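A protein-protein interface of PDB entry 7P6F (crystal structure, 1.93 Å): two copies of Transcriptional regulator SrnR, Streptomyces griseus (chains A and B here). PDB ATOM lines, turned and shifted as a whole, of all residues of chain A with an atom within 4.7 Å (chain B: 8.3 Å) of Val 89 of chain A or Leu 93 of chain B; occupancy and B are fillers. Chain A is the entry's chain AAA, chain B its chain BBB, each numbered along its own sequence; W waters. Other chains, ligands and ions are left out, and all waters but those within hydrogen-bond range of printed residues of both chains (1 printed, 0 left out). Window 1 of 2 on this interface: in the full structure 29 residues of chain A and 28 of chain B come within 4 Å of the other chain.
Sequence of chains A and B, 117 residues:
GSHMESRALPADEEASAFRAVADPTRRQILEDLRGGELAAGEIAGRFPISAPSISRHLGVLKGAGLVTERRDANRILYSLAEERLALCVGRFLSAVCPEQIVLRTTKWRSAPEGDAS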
ATOM      1  N   ALA A  17      27.642 -23.042  28.143  1.00  0.00           N
ATOM      2  CA  ALA A  17      26.677 -23.866  27.381  1.00  0.00           C
ATOM      3  C   ALA A  17      26.430 -23.247  26.001  1.00  0.00           C
ATOM      4  O   ALA A  17      26.510 -23.971  24.988  1.00  0.00           O
ATOM      5  CB  ALA A  17      25.370 -24.026  28.137  1.00  0.00           C
ATOM      6  N   PHE A  18      26.215 -21.939  25.921  1.00  0.00           N
ATOM      7  CA  PHE A  18      26.019 -21.211  24.637  1.00  0.00           C
ATOM      8  C   PHE A  18      27.286 -21.274  23.772  1.00  0.00           C
ATOM      9  O   PHE A  18      27.155 -21.456  22.548  1.00  0.00           O
ATOM     10  CB  PHE A  18      25.477 -19.786  24.853  1.00  0.00           C
ATOM     11  CG  PHE A  18      23.974 -19.789  25.027  1.00  0.00           C
ATOM     12  CD1 PHE A  18      23.156 -19.853  23.925  1.00  0.00           C
ATOM     13  CD2 PHE A  18      23.376 -19.707  26.275  1.00  0.00           C
ATOM     14  CE1 PHE A  18      21.774 -19.889  24.061  1.00  0.00           C
ATOM     15  CE2 PHE A  18      21.993 -19.774  26.399  1.00  0.00           C
ATOM     16  CZ  PHE A  18      21.186 -19.836  25.300  1.00  0.00           C
ATOM     17  N   VAL A  21      27.337 -24.943  22.260  1.00  0.00           N
ATOM     18  CA  VAL A  21      26.345 -25.253  21.207  1.00  0.00           C
ATOM     19  C   VAL A  21      26.468 -24.271  20.042  1.00  0.00           C
ATOM     20  O   VAL A  21      25.755 -24.464  19.042  1.00  0.00           O
ATOM     21  CB  VAL A  21      24.917 -25.360  21.764  1.00  0.00           C
ATOM     22  CG1 VAL A  21      24.813 -26.456  22.827  1.00  0.00           C
ATOM     23  CG2 VAL A  21      24.352 -24.049  22.279  1.00  0.00           C
ATOM     24  N   LEU A  85      21.752 -29.267  29.770  1.00  0.00           N
ATOM     25  CA  LEU A  85      21.543 -28.502  28.513  1.00  0.00           C
ATOM     26  C   LEU A  85      20.171 -27.797  28.577  1.00  0.00           C
ATOM     27  O   LEU A  85      20.083 -26.597  28.182  1.00  0.00           O
ATOM     28  CB  LEU A  85      21.661 -29.469  27.329  1.00  0.00           C
ATOM     29  CG  LEU A  85      21.379 -28.864  25.983  1.00  0.00           C
ATOM     30  CD1 LEU A  85      22.376 -27.747  25.649  1.00  0.00           C
ATOM     31  CD2 LEU A  85      21.391 -29.944  24.933  1.00  0.00           C
ATOM     32  N   ALA A  86      19.103 -28.504  29.008  1.00  0.00           N
ATOM     33  CA  ALA A  86      17.754 -27.911  28.961  1.00  0.00           C
ATOM     34  C   ALA A  86      17.718 -26.665  29.864  1.00  0.00           C
ATOM     35  O   ALA A  86      17.105 -25.662  29.447  1.00  0.00           O
ATOM     36  CB  ALA A  86      16.678 -28.912  29.306  1.00  0.00           C
ATOM     37  N   LEU A  87      18.355 -26.703  31.039  1.00  0.00           N
ATOM     38  CA  LEU A  87      18.277 -25.569  31.994  1.00  0.00           C
ATOM     39  C   LEU A  87      19.142 -24.420  31.473  1.00  0.00           C
ATOM     40  O   LEU A  87      18.618 -23.261  31.405  1.00  0.00           O
ATOM     41  CB  LEU A  87      18.698 -26.012  33.393  1.00  0.00           C
ATOM     42  CG  LEU A  87      18.617 -24.876  34.437  1.00  0.00           C
ATOM     43  CD1 LEU A  87      17.189 -24.258  34.441  1.00  0.00           C
ATOM     44  CD2 LEU A  87      18.971 -25.375  35.836  1.00  0.00           C
ATOM     45  N   CYS A  88      20.365 -24.718  31.031  1.00  0.00           N
ATOM     46  CA  CYS A  88      21.359 -23.683  30.626  1.00  0.00           C
ATOM     47  C   CYS A  88      20.947 -22.962  29.356  1.00  0.00           C
ATOM     48  O   CYS A  88      21.176 -21.743  29.291  1.00  0.00           O
ATOM     49  CB  CYS A  88      22.749 -24.236  30.458  1.00  0.00           C
ATOM     50  SG  CYS A  88      23.421 -24.723  32.050  1.00  0.00           S
ATOM     51  N   VAL A  89      20.344 -23.652  28.386  1.00  0.00           N
ATOM     52  CA  VAL A  89      19.942 -22.961  27.131  1.00  0.00           C
ATOM     53  C   VAL A  89      18.459 -22.625  27.189  1.00  0.00           C
ATOM     54  O   VAL A  89      18.078 -21.520  26.683  1.00  0.00           O
ATOM     55  CB  VAL A  89      20.350 -23.807  25.910  1.00  0.00           C
ATOM     56  CG1 VAL A  89      19.852 -23.187  24.617  1.00  0.00           C
ATOM     57  CG2 VAL A  89      21.838 -24.025  25.901  1.00  0.00           C
ATOM     58  N   GLY A  90      17.652 -23.515  27.787  1.00  0.00           N
ATOM     59  CA  GLY A  90      16.176 -23.438  27.830  1.00  0.00           C
ATOM     60  C   GLY A  90      15.639 -22.348  28.755  1.00  0.00           C
ATOM     61  O   GLY A  90      14.540 -21.810  28.459  1.00  0.00           O
ATOM     62  N   ARG A  91      16.333 -21.995  29.842  1.00  0.00           N
ATOM     63  CA  ARG A  91      15.867 -20.841  30.650  1.00  0.00           C
ATOM     64  C   ARG A  91      15.875 -19.615  29.732  1.00  0.00           C
ATOM     65  O   ARG A  91      14.846 -18.975  29.653  1.00  0.00           O
ATOM     66  CB  ARG A  91      16.625 -20.666  31.977  1.00  0.00           C
ATOM     67  CG  ARG A  91      16.424 -19.281  32.572  1.00  0.00           C
ATOM     68  CD  ARG A  91      17.102 -19.193  33.907  1.00  0.00           C
ATOM     69  NE  ARG A  91      16.320 -19.859  34.931  1.00  0.00           N
ATOM     70  CZ  ARG A  91      16.821 -20.639  35.886  1.00  0.00           C
ATOM     71  NH1 ARG A  91      18.114 -20.881  35.966  1.00  0.00           N
ATOM     72  NH2 ARG A  91      16.013 -21.151  36.792  1.00  0.00           N
ATOM     73  N   PHE A  92      17.020 -19.253  29.130  1.00  0.00           N
ATOM     74  CA  PHE A  92      17.086 -18.120  28.184  1.00  0.00           C
ATOM     75  C   PHE A  92      15.990 -18.275  27.131  1.00  0.00           C
ATOM     76  O   PHE A  92      15.334 -17.271  26.767  1.00  0.00           O
ATOM     77  CB  PHE A  92      18.486 -17.993  27.570  1.00  0.00           C
ATOM     78  CG  PHE A  92      18.541 -17.099  26.366  1.00  0.00           C
ATOM     79  CD1 PHE A  92      18.696 -15.738  26.515  1.00  0.00           C
ATOM     80  CD2 PHE A  92      18.404 -17.622  25.078  1.00  0.00           C
ATOM     81  CE1 PHE A  92      18.746 -14.896  25.417  1.00  0.00           C
ATOM     82  CE2 PHE A  92      18.437 -16.773  23.979  1.00  0.00           C
ATOM     83  CZ  PHE A  92      18.575 -15.415  24.161  1.00  0.00           C
ATOM     84  N   LEU A  93      15.866 -19.452  26.514  1.00  0.00           N
ATOM     85  CA  LEU A  93      15.040 -19.546  25.296  1.00  0.00           C
ATOM     86  C   LEU A  93      13.565 -19.372  25.719  1.00  0.00           C
ATOM     87  O   LEU A  93      12.786 -18.635  24.990  1.00  0.00           O
ATOM     88  CB  LEU A  93      15.284 -20.880  24.561  1.00  0.00           C
ATOM     89  CG  LEU A  93      14.653 -20.962  23.159  1.00  0.00           C
ATOM     90  CD1 LEU A  93      15.299 -19.958  22.233  1.00  0.00           C
ATOM     91  CD2 LEU A  93      14.787 -22.357  22.540  1.00  0.00           C
ATOM     92  N   GLU B  14      19.651 -22.093  11.296  1.00  0.00           N
ATOM     93  CA  GLU B  14      19.966 -22.694  12.616  1.00  0.00           C
ATOM     94  C   GLU B  14      21.402 -22.279  12.989  1.00  0.00           C
ATOM     95  O   GLU B  14      21.641 -21.801  14.172  1.00  0.00           O
ATOM     96  CB  GLU B  14      19.834 -24.220  12.625  1.00  0.00           C
ATOM     97  CG  GLU B  14      20.407 -24.890  13.903  1.00  0.00           C
ATOM     98  CD  GLU B  14      20.336 -26.430  14.004  1.00  0.00           C
ATOM     99  OE1 GLU B  14      19.222 -26.972  13.904  1.00  0.00           O
ATOM    100  OE2 GLU B  14      21.408 -27.091  14.283  1.00  0.00           O
ATOM    101  N   PHE B  18      22.648 -19.777  16.161  1.00  0.00           N
ATOM    102  CA  PHE B  18      23.527 -20.298  17.245  1.00  0.00           C
ATOM    103  C   PHE B  18      24.795 -19.442  17.390  1.00  0.00           C
ATOM    104  O   PHE B  18      25.197 -19.156  18.531  1.00  0.00           O
ATOM    105  CB  PHE B  18      23.787 -21.799  17.077  1.00  0.00           C
ATOM    106  CG  PHE B  18      22.705 -22.643  17.724  1.00  0.00           C
ATOM    107  CD1 PHE B  18      22.661 -22.798  19.106  1.00  0.00           C
ATOM    108  CD2 PHE B  18      21.792 -23.351  16.962  1.00  0.00           C
ATOM    109  CE1 PHE B  18      21.670 -23.564  19.707  1.00  0.00           C
ATOM    110  CE2 PHE B  18      20.816 -24.139  17.569  1.00  0.00           C
ATOM    111  CZ  PHE B  18      20.739 -24.218  18.941  1.00  0.00           C
ATOM    112  N   VAL B  21      23.429 -16.156  19.180  1.00  0.00           N
ATOM    113  CA  VAL B  21      23.141 -16.314  20.643  1.00  0.00           C
ATOM    114  C   VAL B  21      24.375 -16.834  21.395  1.00  0.00           C
ATOM    115  O   VAL B  21      24.300 -16.914  22.627  1.00  0.00           O
ATOM    116  CB  VAL B  21      21.870 -17.143  20.934  1.00  0.00           C
ATOM    117  CG1 VAL B  21      20.652 -16.434  20.339  1.00  0.00           C
ATOM    118  CG2 VAL B  21      21.999 -18.585  20.509  1.00  0.00           C
ATOM    119  N   ARG B  27      22.636 -12.051  23.757  1.00  0.00           N
ATOM    120  CA  ARG B  27      21.514 -12.640  24.512  1.00  0.00           C
ATOM    121  C   ARG B  27      20.833 -11.545  25.368  1.00  0.00           C
ATOM    122  O   ARG B  27      19.591 -11.515  25.423  1.00  0.00           O
ATOM    123  CB  ARG B  27      22.041 -13.780  25.383  1.00  0.00           C
ATOM    124  CG  ARG B  27      22.495 -15.001  24.579  1.00  0.00           C
ATOM    125  CD  ARG B  27      22.576 -16.227  25.497  1.00  0.00           C
ATOM    126  NE  ARG B  27      23.594 -16.134  26.539  1.00  0.00           N
ATOM    127  CZ  ARG B  27      24.911 -16.239  26.371  1.00  0.00           C
ATOM    128  NH1 ARG B  27      25.417 -16.458  25.178  1.00  0.00           N
ATOM    129  NH2 ARG B  27      25.737 -16.164  27.393  1.00  0.00           N
ATOM    130  N   ALA B  86      12.738 -19.061  18.194  1.00  0.00           N
ATOM    131  CA  ALA B  86      12.134 -20.243  18.845  1.00  0.00           C
ATOM    132  C   ALA B  86      12.385 -21.477  17.959  1.00  0.00           C
ATOM    133  O   ALA B  86      12.813 -22.508  18.475  1.00  0.00           O
ATOM    134  CB  ALA B  86      10.652 -20.027  19.074  1.00  0.00           C
ATOM    135  N   LEU B  87      12.166 -21.366  16.652  1.00  0.00           N
ATOM    136  CA  LEU B  87      12.335 -22.505  15.709  1.00  0.00           C
ATOM    137  C   LEU B  87      13.835 -22.764  15.502  1.00  0.00           C
ATOM    138  O   LEU B  87      14.233 -23.946  15.571  1.00  0.00           O
ATOM    139  CB  LEU B  87      11.651 -22.159  14.382  1.00  0.00           C
ATOM    140  CG  LEU B  87      11.687 -23.267  13.328  1.00  0.00           C
ATOM    141  CD1 LEU B  87      11.080 -24.531  13.905  1.00  0.00           C
ATOM    142  CD2 LEU B  87      10.931 -22.863  12.058  1.00  0.00           C
ATOM    143  N   CYS B  88      14.648 -21.732  15.244  1.00  0.00           N
ATOM    144  CA  CYS B  88      16.079 -21.936  14.878  1.00  0.00           C
ATOM    145  C   CYS B  88      16.828 -22.558  16.049  1.00  0.00           C
ATOM    146  O   CYS B  88      17.634 -23.456  15.810  1.00  0.00           O
ATOM    147  CB  CYS B  88      16.758 -20.668  14.396  1.00  0.00           C
ATOM    148  SG  CYS B  88      16.107 -20.092  12.801  1.00  0.00           S
ATOM    149  N   VAL B  89      16.548 -22.158  17.295  1.00  0.00           N
ATOM    150  CA  VAL B  89      17.230 -22.748  18.468  1.00  0.00           C
ATOM    151  C   VAL B  89      16.379 -23.844  19.082  1.00  0.00           C
ATOM    152  O   VAL B  89      16.984 -24.853  19.497  1.00  0.00           O
ATOM    153  CB  VAL B  89      17.636 -21.673  19.493  1.00  0.00           C
ATOM    154  CG1 VAL B  89      18.166 -22.288  20.778  1.00  0.00           C
ATOM    155  CG2 VAL B  89      18.635 -20.712  18.860  1.00  0.00           C
ATOM    156  N   GLY B  90      15.052 -23.683  19.100  1.00  0.00           N
ATOM    157  CA  GLY B  90      14.113 -24.587  19.793  1.00  0.00           C
ATOM    158  C   GLY B  90      13.975 -25.939  19.107  1.00  0.00           C
ATOM    159  O   GLY B  90      13.762 -26.931  19.829  1.00  0.00           O
ATOM    160  N   ARG B  91      14.149 -26.051  17.794  1.00  0.00           N
ATOM    161  CA  ARG B  91      14.025 -27.402  17.164  1.00  0.00           C
ATOM    162  C   ARG B  91      15.166 -28.248  17.726  1.00  0.00           C
ATOM    163  O   ARG B  91      14.952 -29.379  18.158  1.00  0.00           O
ATOM    164  CB  ARG B  91      14.027 -27.335  15.632  1.00  0.00           C
ATOM    165  CG  ARG B  91      14.463 -28.635  14.971  1.00  0.00           C
ATOM    166  CD  ARG B  91      14.285 -28.531  13.488  1.00  0.00           C
ATOM    167  NE  ARG B  91      12.887 -28.587  13.042  1.00  0.00           N
ATOM    168  CZ  ARG B  91      12.347 -27.834  12.086  1.00  0.00           C
ATOM    169  NH1 ARG B  91      13.015 -26.848  11.524  1.00  0.00           N
ATOM    170  NH2 ARG B  91      11.107 -28.040  11.697  1.00  0.00           N
ATOM    171  N   PHE B  92      16.399 -27.726  17.662  1.00  0.00           N
ATOM    172  CA  PHE B  92      17.574 -28.465  18.153  1.00  0.00           C
ATOM    173  C   PHE B  92      17.339 -28.797  19.645  1.00  0.00           C
ATOM    174  O   PHE B  92      17.598 -29.923  20.088  1.00  0.00           O
ATOM    175  CB  PHE B  92      18.856 -27.658  17.929  1.00  0.00           C
ATOM    176  CG  PHE B  92      19.968 -28.167  18.785  1.00  0.00           C
ATOM    177  CD1 PHE B  92      20.759 -29.207  18.341  1.00  0.00           C
ATOM    178  CD2 PHE B  92      20.210 -27.598  20.023  1.00  0.00           C
ATOM    179  CE1 PHE B  92      21.806 -29.682  19.116  1.00  0.00           C
ATOM    180  CE2 PHE B  92      21.261 -28.070  20.795  1.00  0.00           C
ATOM    181  CZ  PHE B  92      22.050 -29.110  20.341  1.00  0.00           C
ATOM    182  N   LEU B  93      16.940 -27.805  20.444  1.00  0.00           N
ATOM    183  CA  LEU B  93      16.912 -27.996  21.914  1.00  0.00           C
ATOM    184  C   LEU B  93      15.831 -29.035  22.280  1.00  0.00           C
ATOM    185  O   LEU B  93      16.143 -29.882  23.145  1.00  0.00           O
ATOM    186  CB  LEU B  93      16.732 -26.640  22.635  1.00  0.00           C
ATOM    187  CG  LEU B  93      17.036 -26.668  24.135  1.00  0.00           C
ATOM    188  CD1 LEU B  93      18.504 -26.984  24.420  1.00  0.00           C
ATOM    189  CD2 LEU B  93      16.602 -25.341  24.804  1.00  0.00           C
ATOM    190  N   SER B  94      14.661 -29.000  21.626  1.00  0.00           N
ATOM    191  CA  SER B  94      13.549 -29.961  21.831  1.00  0.00           C
ATOM    192  C   SER B  94      13.927 -31.326  21.239  1.00  0.00           C
ATOM    193  O   SER B  94      13.407 -32.301  21.714  1.00  0.00           O
ATOM    194  CB  SER B  94      12.231 -29.464  21.290  1.00  0.00           C
ATOM    195  OG  SER B  94      12.291 -29.206  19.897  1.00  0.00           O
ATOM    196  N   ALA B  95      14.808 -31.376  20.242  1.00  0.00           N
ATOM    197  CA  ALA B  95      15.297 -32.670  19.682  1.00  0.00           C
ATOM    198  C   ALA B  95      16.212 -33.350  20.687  1.00  0.00           C
ATOM    199  O   ALA B  95      16.127 -34.592  20.842  1.00  0.00           O
ATOM    200  CB  ALA B  95      16.027 -32.473  18.373  1.00  0.00           C
ATOM    201  N   VAL B  96      17.093 -32.585  21.328  1.00  0.00           N
ATOM    202  CA  VAL B  96      18.115 -33.160  22.243  1.00  0.00           C
ATOM    203  C   VAL B  96      17.485 -33.338  23.626  1.00  0.00           C
ATOM    204  O   VAL B  96      17.934 -34.279  24.343  1.00  0.00           O
ATOM    205  CB  VAL B  96      19.411 -32.328  22.220  1.00  0.00           C
ATOM    206  CG1 VAL B  96      20.362 -32.758  23.298  1.00  0.00           C
ATOM    207  CG2 VAL B  96      20.107 -32.473  20.880  1.00  0.00           C
ATOM    208  N   CYS B  97      16.534 -32.470  24.021  1.00  0.00           N
ATOM    209  CA  CYS B  97      15.929 -32.513  25.370  1.00  0.00           C
ATOM    210  C   CYS B  97      14.413 -32.679  25.292  1.00  0.00           C
ATOM    211  O   CYS B  97      13.662 -31.867  25.890  1.00  0.00           O
ATOM    212  CB  CYS B  97      16.231 -31.235  26.153  1.00  0.00           C
ATOM    213  SG  CYS B  97      17.984 -30.771  26.110  1.00  0.00           S
ATOM    214  N   PRO B  98      13.913 -33.736  24.605  1.00  0.00           N
ATOM    215  CA  PRO B  98      12.477 -33.899  24.418  1.00  0.00           C
ATOM    216  C   PRO B  98      11.685 -33.940  25.738  1.00  0.00           C
ATOM    217  O   PRO B  98      10.526 -33.561  25.711  1.00  0.00           O
ATOM    218  CB  PRO B  98      12.340 -35.258  23.725  1.00  0.00           C
ATOM    219  CG  PRO B  98      13.635 -35.974  24.013  1.00  0.00           C
ATOM    220  CD  PRO B  98      14.672 -34.873  24.059  1.00  0.00           C
ATOM    221  N   GLU B  99      12.298 -34.398  26.816  1.00  0.00           N
ATOM    222  CA  GLU B  99      11.581 -34.565  28.112  1.00  0.00           C
ATOM    223  C   GLU B  99      11.459 -33.203  28.782  1.00  0.00           C
ATOM    224  O   GLU B  99      10.475 -33.011  29.549  1.00  0.00           O
ATOM    225  CB  GLU B  99      12.262 -35.612  29.004  1.00  0.00           C
ATOM    226  CG  GLU B  99      11.914 -37.053  28.644  1.00  0.00           C
ATOM    227  CD  GLU B  99      10.431 -37.287  28.363  1.00  0.00           C
ATOM    228  OE1 GLU B  99       9.596 -37.172  29.313  1.00  0.00           O
ATOM    229  OE2 GLU B  99      10.088 -37.562  27.191  1.00  0.00           O
ATOM    230  N   GLN B 100      12.332 -32.236  28.459  1.00  0.00           N
ATOM    231  CA  GLN B 100      12.397 -30.979  29.253  1.00  0.00           C
ATOM    232  C   GLN B 100      11.992 -29.741  28.434  1.00  0.00           C
ATOM    233  O   GLN B 100      11.767 -28.700  29.044  1.00  0.00           O
ATOM    234  CB  GLN B 100      13.799 -30.725  29.816  1.00  0.00           C
ATOM    235  CG  GLN B 100      14.294 -31.727  30.837  1.00  0.00           C
ATOM    236  CD  GLN B 100      14.898 -32.983  30.259  1.00  0.00           C
ATOM    237  OE1 GLN B 100      15.178 -33.103  29.061  1.00  0.00           O
ATOM    238  NE2 GLN B 100      15.053 -33.971  31.128  1.00  0.00           N
ATOM    239  N   ILE B 101      11.923 -29.812  27.106  1.00  0.00           N
ATOM    240  CA  ILE B 101      11.805 -28.624  26.233  1.00  0.00           C
ATOM    241  C   ILE B 101      10.729 -28.919  25.213  1.00  0.00           C
ATOM    242  O   ILE B 101      10.901 -29.893  24.461  1.00  0.00           O
ATOM    243  CB  ILE B 101      13.140 -28.268  25.571  1.00  0.00           C
ATOM    244  CG1 ILE B 101      14.246 -27.918  26.571  1.00  0.00           C
ATOM    245  CG2 ILE B 101      12.928 -27.143  24.593  1.00  0.00           C
ATOM    246  CD1 ILE B 101      13.985 -26.636  27.369  1.00  0.00           C
ATOM    247  N   VAL B 102       9.673 -28.119  25.211  1.00  0.00           N
ATOM    248  CA  VAL B 102       8.570 -28.266  24.243  1.00  0.00           C
ATOM    249  C   VAL B 102       8.462 -27.034  23.377  1.00  0.00           C
ATOM    250  O   VAL B 102       8.403 -25.914  23.924  1.00  0.00           O
ATOM    251  CB  VAL B 102       7.246 -28.544  24.952  1.00  0.00           C
ATOM    252  CG1 VAL B 102       6.133 -28.707  23.943  1.00  0.00           C
ATOM    253  CG2 VAL B 102       7.374 -29.771  25.833  1.00  0.00           C
ATOM    254  N   LEU B 103       8.470 -27.266  22.066  1.00  0.00           N
ATOM    255  CA  LEU B 103       8.363 -26.188  21.075  1.00  0.00           C
ATOM    256  C   LEU B 103       6.951 -26.182  20.500  1.00  0.00           C
ATOM    257  O   LEU B 103       6.558 -27.219  19.957  1.00  0.00           O
ATOM    258  CB  LEU B 103       9.421 -26.406  20.002  1.00  0.00           C
ATOM    259  CG  LEU B 103       9.185 -25.587  18.755  1.00  0.00           C
ATOM    260  CD1 LEU B 103       9.247 -24.119  19.079  1.00  0.00           C
ATOM    261  CD2 LEU B 103      10.147 -25.938  17.632  1.00  0.00           C
HETATM  262  O   HOH W   1      24.962 -20.701  20.881  1.00  0.00           O
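The backbone carbonyl oxygen of Leu 93 of chain B lies close to the side-chain sulfur of Cys 97 of chain B, at 3.6 Å. The backbone carbonyl oxygen (O) of Val 21 of chain B lies within hydrogen-bond range of the guanidinium group (NH1) of Arg 27 of chain B, at 2.8 Å. The backbone carbonyl oxygen (O) of Gly 90 of chain B is in hydrogen-bond range of the side-chain hydroxyl (OG) of Ser 94 of chain B (2.7 Å).
Among the printed residues, merely in contact across the chains: Phe 18 of chain A with Val 21 of chain B (3.4 Å), Phe 18 of chain A with Arg 27 of chain B (3.3 Å), Val 21 of chain A with Phe 18 of chain B (3.5 Å), Leu 85 of chain A with Leu 93 of chain B (3.8 Å), Leu 85 of chain A with Val 96 of chain B (3.4 Å), Leu 85 of chain A with Cys 97 of chain B (3.7 Å), Ala 86 of chain A with Cys 97 of chain B (3.8 Å), Ala 86 of chain A with Gln 100 of chain B (3.4 Å), Ala 86 of chain A with Ile 101 of chain B (3.8 Å), Val 89 of chain A with Leu 93 of chain B (3.9 Å), Gly 90 of chain A with Leu 93 of chain B (3.6 Å), Gly 90 of chain A with Ile 101 of chain B (3.9 Å), Phe 92 of chain A with Arg 27 of chain B (3.5 Å), Leu 93 of chain A with Val 89 of chain B (3.8 Å) and Leu 93 of chain A with Gly 90 of chain B (3.6 Å).
Printed residues of chain B within 4 Å of Leu 85 of chain A: Leu 93 (3.8 Å), Val 96 (3.4 Å) and Cys 97 (3.7 Å). Of the printed residues of chain B, Ala 86 of chain A touches Cys 97 (3.8 Å), Gln 100 (3.4 Å) and Ile 101 (3.8 Å). Val 89 of chain A touches one residue of chain B. Gly 90 of chain A touches just these residues of chain B: Leu 93 (3.6 Å) and Ile 101 (3.9 Å). Of the printed residues of chain B, Phe 92 of chain A touches Arg 27 (3.5 Å). Of the printed residues of chain A, Val 21 of chain B touches Phe 18 (3.4 Å). Ala 86 of chain B touches none of the printed residues of chain A. Leu 93 of chain B touches three residues of chain A. Of the printed residues of chain A, Cys 97 of chain B touches Leu 85 and Ala 86. The nearest residue of chain B that does not touch Val 89 of chain A is Val 89 of chain B (4.3 Å). The nearest residue of chain A that does not touch Leu 93 of chain B is Leu 93 of chain A (4.2 Å).
Of the 12 printed residues of chain A, 8 touch a printed residue of chain B. Hydrophobic or aromatic side chains of chain B that line the printed part of chain A: Phe 18, Val 21, Val 89, Leu 93, Val 96 and Ile 101. Among the printed residues, 15 pairs touch across the chains.
Phe 18 of chain A touches Val 21 of chain B, and with the chains exchanged Val 21 of chain A touches Phe 18 of chain B. Val 89 of chain A touches Leu 93 of chain B, and with the chains exchanged Leu 93 of chain A touches Val 89 of chain B. Gly 90 of chain A touches Leu 93 of chain B, and with the chains exchanged Leu 93 of chain A touches Gly 90 of chain B. Of the 15 pairs that touch across the chains among the printed residues, 6 have their exchanged pair printed and touching as well.
Water W1 bridges O of Phe 18 of chain B and O of Phe 18 of chain A.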
